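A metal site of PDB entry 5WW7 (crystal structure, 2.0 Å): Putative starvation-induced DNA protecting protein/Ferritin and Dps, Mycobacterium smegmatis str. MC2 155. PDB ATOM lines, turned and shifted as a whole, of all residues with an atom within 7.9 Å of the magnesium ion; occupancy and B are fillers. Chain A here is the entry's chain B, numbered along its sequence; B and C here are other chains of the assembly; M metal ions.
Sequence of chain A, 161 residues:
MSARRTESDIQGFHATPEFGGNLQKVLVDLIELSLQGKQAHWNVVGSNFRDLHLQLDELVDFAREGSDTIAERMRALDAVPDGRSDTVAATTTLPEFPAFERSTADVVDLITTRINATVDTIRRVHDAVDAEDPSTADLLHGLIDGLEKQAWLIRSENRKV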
ATOM      1  N   SER A  47      13.621  -4.526  22.597  1.00  0.00           N
ATOM      2  CA  SER A  47      13.420  -4.055  21.230  1.00  0.00           C
ATOM      3  C   SER A  47      12.240  -4.759  20.572  1.00  0.00           C
ATOM      4  O   SER A  47      12.104  -5.979  20.641  1.00  0.00           O
ATOM      5  CB  SER A  47      14.680  -4.242  20.400  1.00  0.00           C
ATOM      6  OG  SER A  47      14.975  -5.620  20.289  1.00  0.00           O
ATOM      7  N   ASN A  48      11.388  -3.940  19.952  1.00  0.00           N
ATOM      8  CA  ASN A  48      10.130  -4.362  19.328  1.00  0.00           C
ATOM      9  C   ASN A  48       9.106  -4.909  20.328  1.00  0.00           C
ATOM     10  O   ASN A  48       8.313  -5.792  20.006  1.00  0.00           O
ATOM     11  CB  ASN A  48      10.354  -5.332  18.165  1.00  0.00           C
ATOM     12  CG  ASN A  48       9.232  -5.279  17.160  1.00  0.00           C
ATOM     13  OD1 ASN A  48       8.539  -4.259  17.042  1.00  0.00           O
ATOM     14  ND2 ASN A  48       9.035  -6.372  16.426  1.00  0.00           N
ATOM     15  N   PHE A  49       9.128  -4.342  21.537  1.00  0.00           N
ATOM     16  CA  PHE A  49       8.161  -4.640  22.586  1.00  0.00           C
ATOM     17  C   PHE A  49       6.724  -4.634  22.083  1.00  0.00           C
ATOM     18  O   PHE A  49       5.971  -5.583  22.310  1.00  0.00           O
ATOM     19  CB  PHE A  49       8.273  -3.641  23.766  1.00  0.00           C
ATOM     20  CG  PHE A  49       7.078  -3.673  24.679  1.00  0.00           C
ATOM     21  CD1 PHE A  49       6.931  -4.713  25.611  1.00  0.00           C
ATOM     22  CD2 PHE A  49       6.079  -2.699  24.596  1.00  0.00           C
ATOM     23  CE1 PHE A  49       5.809  -4.765  26.447  1.00  0.00           C
ATOM     24  CE2 PHE A  49       4.968  -2.751  25.423  1.00  0.00           C
ATOM     25  CZ  PHE A  49       4.836  -3.776  26.350  1.00  0.00           C
ATOM     26  N   ARG A  50       6.340  -3.545  21.418  1.00  0.00           N
ATOM     27  CA  ARG A  50       4.940  -3.289  21.127  1.00  0.00           C
ATOM     28  C   ARG A  50       4.326  -4.367  20.220  1.00  0.00           C
ATOM     29  O   ARG A  50       3.289  -4.930  20.562  1.00  0.00           O
ATOM     30  CB  ARG A  50       4.718  -1.875  20.584  1.00  0.00           C
ATOM     31  CG  ARG A  50       3.270  -1.556  20.305  1.00  0.00           C
ATOM     32  CD  ARG A  50       3.099  -0.108  19.896  1.00  0.00           C
ATOM     33  NE  ARG A  50       1.688   0.217  19.665  1.00  0.00           N
ATOM     34  CZ  ARG A  50       1.019   0.018  18.530  1.00  0.00           C
ATOM     35  NH1 ARG A  50       1.603  -0.548  17.472  1.00  0.00           N
ATOM     36  NH2 ARG A  50      -0.260   0.367  18.481  1.00  0.00           N
ATOM     37  N   ASP A  51       5.003  -4.659  19.104  1.00  0.00           N
ATOM     38  CA  ASP A  51       4.603  -5.729  18.184  1.00  0.00           C
ATOM     39  C   ASP A  51       4.434  -7.068  18.885  1.00  0.00           C
ATOM     40  O   ASP A  51       3.480  -7.788  18.594  1.00  0.00           O
ATOM     41  CB  ASP A  51       5.616  -5.883  17.052  1.00  0.00           C
ATOM     42  CG  ASP A  51       5.297  -5.025  15.841  1.00  0.00           C
ATOM     43  OD1 ASP A  51       4.120  -4.799  15.507  1.00  0.00           O
ATOM     44  OD2 ASP A  51       6.264  -4.573  15.198  1.00  0.00           O
ATOM     45  N   LEU A  52       5.368  -7.417  19.777  1.00  0.00           N
ATOM     46  CA  LEU A  52       5.274  -8.675  20.532  1.00  0.00           C
ATOM     47  C   LEU A  52       4.137  -8.665  21.528  1.00  0.00           C
ATOM     48  O   LEU A  52       3.348  -9.613  21.556  1.00  0.00           O
ATOM     49  CB  LEU A  52       6.604  -9.037  21.221  1.00  0.00           C
ATOM     50  CG  LEU A  52       7.569 -10.012  20.535  1.00  0.00           C
ATOM     51  CD1 LEU A  52       6.904 -11.372  20.276  1.00  0.00           C
ATOM     52  CD2 LEU A  52       8.165  -9.436  19.243  1.00  0.00           C
ATOM     53  N   GLU A 157      10.403 -12.841  13.651  1.00  0.00           N
ATOM     54  CA  GLU A 157      11.135 -11.778  14.376  1.00  0.00           C
ATOM     55  C   GLU A 157      12.610 -12.125  14.647  1.00  0.00           C
ATOM     56  O   GLU A 157      13.471 -11.234  14.614  1.00  0.00           O
ATOM     57  CB  GLU A 157      10.401 -11.434  15.691  1.00  0.00           C
ATOM     58  CG  GLU A 157      11.094 -10.413  16.614  1.00  0.00           C
ATOM     59  CD  GLU A 157      11.075  -8.983  16.091  1.00  0.00           C
ATOM     60  OE1 GLU A 157      11.932  -8.171  16.514  1.00  0.00           O
ATOM     61  OE2 GLU A 157      10.206  -8.649  15.262  1.00  0.00           O
ATOM     62  N   SER B  47      14.190  -8.631  12.401  1.00  0.00           N
ATOM     63  CA  SER B  47      13.843  -7.612  13.398  1.00  0.00           C
ATOM     64  C   SER B  47      12.744  -6.683  12.900  1.00  0.00           C
ATOM     65  O   SER B  47      12.836  -6.155  11.815  1.00  0.00           O
ATOM     66  CB  SER B  47      15.065  -6.764  13.771  1.00  0.00           C
ATOM     67  OG  SER B  47      16.027  -7.579  14.396  1.00  0.00           O
ATOM     68  N   ASN B  48      11.731  -6.496  13.749  1.00  0.00           N
ATOM     69  CA  ASN B  48      10.541  -5.698  13.435  1.00  0.00           C
ATOM     70  C   ASN B  48       9.712  -6.244  12.253  1.00  0.00           C
ATOM     71  O   ASN B  48       9.136  -5.478  11.462  1.00  0.00           O
ATOM     72  CB  ASN B  48      10.876  -4.201  13.262  1.00  0.00           C
ATOM     73  CG  ASN B  48       9.694  -3.314  13.578  1.00  0.00           C
ATOM     74  OD1 ASN B  48       8.802  -3.714  14.328  1.00  0.00           O
ATOM     75  ND2 ASN B  48       9.658  -2.122  12.997  1.00  0.00           N
ATOM     76  N   PHE B  49       9.652  -7.582  12.164  1.00  0.00           N
ATOM     77  CA  PHE B  49       8.864  -8.299  11.158  1.00  0.00           C
ATOM     78  C   PHE B  49       7.412  -7.801  11.101  1.00  0.00           C
ATOM     79  O   PHE B  49       6.894  -7.499  10.034  1.00  0.00           O
ATOM     80  CB  PHE B  49       8.860  -9.822  11.415  1.00  0.00           C
ATOM     81  CG  PHE B  49       7.765 -10.556  10.662  1.00  0.00           C
ATOM     82  CD1 PHE B  49       6.571 -10.929  11.317  1.00  0.00           C
ATOM     83  CD2 PHE B  49       7.911 -10.849   9.308  1.00  0.00           C
ATOM     84  CE1 PHE B  49       5.563 -11.586  10.623  1.00  0.00           C
ATOM     85  CE2 PHE B  49       6.897 -11.509   8.607  1.00  0.00           C
ATOM     86  CZ  PHE B  49       5.721 -11.882   9.274  1.00  0.00           C
ATOM     87  N   ARG B  50       6.751  -7.762  12.260  1.00  0.00           N
ATOM     88  CA  ARG B  50       5.306  -7.515  12.307  1.00  0.00           C
ATOM     89  C   ARG B  50       4.935  -6.144  11.726  1.00  0.00           C
ATOM     90  O   ARG B  50       4.053  -6.057  10.879  1.00  0.00           O
ATOM     91  CB  ARG B  50       4.753  -7.710  13.724  1.00  0.00           C
ATOM     92  CG  ARG B  50       3.243  -7.609  13.817  1.00  0.00           C
ATOM     93  CD  ARG B  50       2.746  -7.917  15.224  1.00  0.00           C
ATOM     94  NE  ARG B  50       1.305  -7.745  15.341  1.00  0.00           N
ATOM     95  CZ  ARG B  50       0.682  -6.590  15.581  1.00  0.00           C
ATOM     96  NH1 ARG B  50       1.348  -5.464  15.737  1.00  0.00           N
ATOM     97  NH2 ARG B  50      -0.648  -6.569  15.660  1.00  0.00           N
ATOM     98  N   ASP B  51       5.626  -5.088  12.176  1.00  0.00           N
ATOM     99  CA  ASP B  51       5.413  -3.731  11.663  1.00  0.00           C
ATOM    100  C   ASP B  51       5.544  -3.659  10.138  1.00  0.00           C
ATOM    101  O   ASP B  51       4.701  -3.056   9.468  1.00  0.00           O
ATOM    102  CB  ASP B  51       6.394  -2.740  12.289  1.00  0.00           C
ATOM    103  CG  ASP B  51       5.832  -2.073  13.542  1.00  0.00           C
ATOM    104  OD1 ASP B  51       4.606  -1.827  13.618  1.00  0.00           O
ATOM    105  OD2 ASP B  51       6.636  -1.807  14.461  1.00  0.00           O
ATOM    106  N   LEU B  52       6.600  -4.288   9.608  1.00  0.00           N
ATOM    107  CA  LEU B  52       6.840  -4.337   8.168  1.00  0.00           C
ATOM    108  C   LEU B  52       5.781  -5.146   7.445  1.00  0.00           C
ATOM    109  O   LEU B  52       5.216  -4.676   6.464  1.00  0.00           O
ATOM    110  CB  LEU B  52       8.241  -4.896   7.860  1.00  0.00           C
ATOM    111  CG  LEU B  52       9.371  -3.907   7.516  1.00  0.00           C
ATOM    112  CD1 LEU B  52       9.045  -3.110   6.256  1.00  0.00           C
ATOM    113  CD2 LEU B  52       9.692  -2.990   8.686  1.00  0.00           C
ATOM    114  N   GLU B 157      12.309   3.297   9.145  1.00  0.00           N
ATOM    115  CA  GLU B 157      12.859   2.116   9.838  1.00  0.00           C
ATOM    116  C   GLU B 157      14.389   1.993   9.738  1.00  0.00           C
ATOM    117  O   GLU B 157      15.047   1.652  10.724  1.00  0.00           O
ATOM    118  CB  GLU B 157      12.195   0.830   9.304  1.00  0.00           C
ATOM    119  CG  GLU B 157      12.689  -0.481   9.923  1.00  0.00           C
ATOM    120  CD  GLU B 157      12.324  -0.657  11.398  1.00  0.00           C
ATOM    121  OE1 GLU B 157      11.287  -0.115  11.855  1.00  0.00           O
ATOM    122  OE2 GLU B 157      13.093  -1.343  12.107  1.00  0.00           O
ATOM    123  N   SER C  47      15.094   2.232  14.096  1.00  0.00           N
ATOM    124  CA  SER C  47      14.633   0.876  14.428  1.00  0.00           C
ATOM    125  C   SER C  47      13.302   0.897  15.170  1.00  0.00           C
ATOM    126  O   SER C  47      13.169   1.572  16.200  1.00  0.00           O
ATOM    127  CB  SER C  47      15.697   0.148  15.259  1.00  0.00           C
ATOM    128  OG  SER C  47      15.501  -1.245  15.208  1.00  0.00           O
ATOM    129  N   ASN C  48      12.324   0.156  14.651  1.00  0.00           N
ATOM    130  CA  ASN C  48      10.978   0.077  15.219  1.00  0.00           C
ATOM    131  C   ASN C  48      10.183   1.391  15.162  1.00  0.00           C
ATOM    132  O   ASN C  48       9.379   1.701  16.062  1.00  0.00           O
ATOM    133  CB  ASN C  48      10.972  -0.521  16.644  1.00  0.00           C
ATOM    134  CG  ASN C  48       9.633  -1.134  17.005  1.00  0.00           C
ATOM    135  OD1 ASN C  48       8.899  -1.554  16.111  1.00  0.00           O
ATOM    136  ND2 ASN C  48       9.300  -1.167  18.297  1.00  0.00           N
ATOM    137  N   PHE C  49      10.426   2.142  14.090  1.00  0.00           N
ATOM    138  CA  PHE C  49       9.725   3.399  13.822  1.00  0.00           C
ATOM    139  C   PHE C  49       8.202   3.271  13.931  1.00  0.00           C
ATOM    140  O   PHE C  49       7.553   4.094  14.565  1.00  0.00           O
ATOM    141  CB  PHE C  49      10.084   3.952  12.432  1.00  0.00           C
ATOM    142  CG  PHE C  49       9.086   4.952  11.918  1.00  0.00           C
ATOM    143  CD1 PHE C  49       9.139   6.292  12.335  1.00  0.00           C
ATOM    144  CD2 PHE C  49       8.069   4.557  11.036  1.00  0.00           C
ATOM    145  CE1 PHE C  49       8.196   7.213  11.878  1.00  0.00           C
ATOM    146  CE2 PHE C  49       7.128   5.476  10.592  1.00  0.00           C
ATOM    147  CZ  PHE C  49       7.194   6.802  11.005  1.00  0.00           C
ATOM    148  N   ARG C  50       7.643   2.253  13.264  1.00  0.00           N
ATOM    149  CA  ARG C  50       6.194   2.170  13.092  1.00  0.00           C
ATOM    150  C   ARG C  50       5.484   2.059  14.449  1.00  0.00           C
ATOM    151  O   ARG C  50       4.567   2.828  14.726  1.00  0.00           O
ATOM    152  CB  ARG C  50       5.804   1.052  12.132  1.00  0.00           C
ATOM    153  CG  ARG C  50       4.310   0.979  11.842  1.00  0.00           C
ATOM    154  CD  ARG C  50       3.980  -0.068  10.790  1.00  0.00           C
ATOM    155  NE  ARG C  50       2.532  -0.145  10.561  1.00  0.00           N
ATOM    156  CZ  ARG C  50       1.676  -0.848  11.304  1.00  0.00           C
ATOM    157  NH1 ARG C  50       2.075  -1.565  12.349  1.00  0.00           N
ATOM    158  NH2 ARG C  50       0.378  -0.829  10.994  1.00  0.00           N
ATOM    159  N   ASP C  51       5.936   1.118  15.293  1.00  0.00           N
ATOM    160  CA  ASP C  51       5.369   0.946  16.643  1.00  0.00           C
ATOM    161  C   ASP C  51       5.383   2.221  17.458  1.00  0.00           C
ATOM    162  O   ASP C  51       4.388   2.548  18.096  1.00  0.00           O
ATOM    163  CB  ASP C  51       6.105  -0.133  17.428  1.00  0.00           C
ATOM    164  CG  ASP C  51       5.505  -1.498  17.241  1.00  0.00           C
ATOM    165  OD1 ASP C  51       4.266  -1.630  17.139  1.00  0.00           O
ATOM    166  OD2 ASP C  51       6.308  -2.454  17.217  1.00  0.00           O
ATOM    167  N   LEU C  52       6.523   2.920  17.434  1.00  0.00           N
ATOM    168  CA  LEU C  52       6.681   4.169  18.185  1.00  0.00           C
ATOM    169  C   LEU C  52       5.793   5.292  17.651  1.00  0.00           C
ATOM    170  O   LEU C  52       5.124   5.953  18.426  1.00  0.00           O
ATOM    171  CB  LEU C  52       8.148   4.615  18.240  1.00  0.00           C
ATOM    172  CG  LEU C  52       8.991   4.192  19.452  1.00  0.00           C
ATOM    173  CD1 LEU C  52       8.374   4.693  20.754  1.00  0.00           C
ATOM    174  CD2 LEU C  52       9.213   2.665  19.504  1.00  0.00           C
ATOM    175  N   GLU C 157      10.405  -0.694  25.368  1.00  0.00           N
ATOM    176  CA  GLU C 157      11.215  -0.743  24.148  1.00  0.00           C
ATOM    177  C   GLU C 157      12.728  -0.688  24.417  1.00  0.00           C
ATOM    178  O   GLU C 157      13.489  -1.400  23.767  1.00  0.00           O
ATOM    179  CB  GLU C 157      10.799   0.384  23.182  1.00  0.00           C
ATOM    180  CG  GLU C 157      11.638   0.523  21.899  1.00  0.00           C
ATOM    181  CD  GLU C 157      11.523  -0.644  20.929  1.00  0.00           C
ATOM    182  OE1 GLU C 157      12.469  -0.859  20.146  1.00  0.00           O
ATOM    183  OE2 GLU C 157      10.494  -1.346  20.934  1.00  0.00           O
HETATM  184 MG    MG M   1       7.616  -3.096  15.749  1.00  0.00          MG
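ND2 of Asn 48 of chain C sits at hydrogen-bond distance from OE2 of Glu 157 of chain C (2.9 Å).
The side-chain amide nitrogen (ND2) of Asn 48 of chain B sits at hydrogen-bond distance from the side-chain carboxylate (OE1) of Glu 157 of chain B.
N of Asn 48 of chain C is in hydrogen-bond range of OE1 of Glu 157 of chain B (3.0 Å).
The side-chain amide nitrogen (ND2) of Asn 48 of chain A is in hydrogen-bond range of the side-chain carboxylate (OE2) of Glu 157 of chain A (2.8 Å).
The side-chain carboxylate (OE2) of Glu 157 of chain A sits at hydrogen-bond distance from the backbone NH (N) of Asn 48 of chain B (3.0 Å).
The backbone NH (N) of Asn 48 of chain A sits at hydrogen-bond distance from the side-chain carboxylate (OE2) of Glu 157 of chain C, 2.9 Å away.
The side-chain carboxylate (OD1) of Asp 51 of chain A is in salt-bridge range of the guanidinium group (NH1) of Arg 50 of chain B.
NH1 of Arg 50 of chain C is in salt-bridge range of OD1 of Asp 51 of chain B (2.8 Å).
The magnesium ion is bound by OD1 of Asn 48 of chain B (2.0 Å), OD1 of Asn 48 of chain A (2.0 Å), OD1 of Asn 48 of chain C (2.0 Å), OD2 of Asp 51 of chain C (2.1 Å), OD2 of Asp 51 of chain B (2.1 Å) and OD2 of Asp 51 of chain A (2.1 Å).
The magnesium ion has six donor atoms within binding distance.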
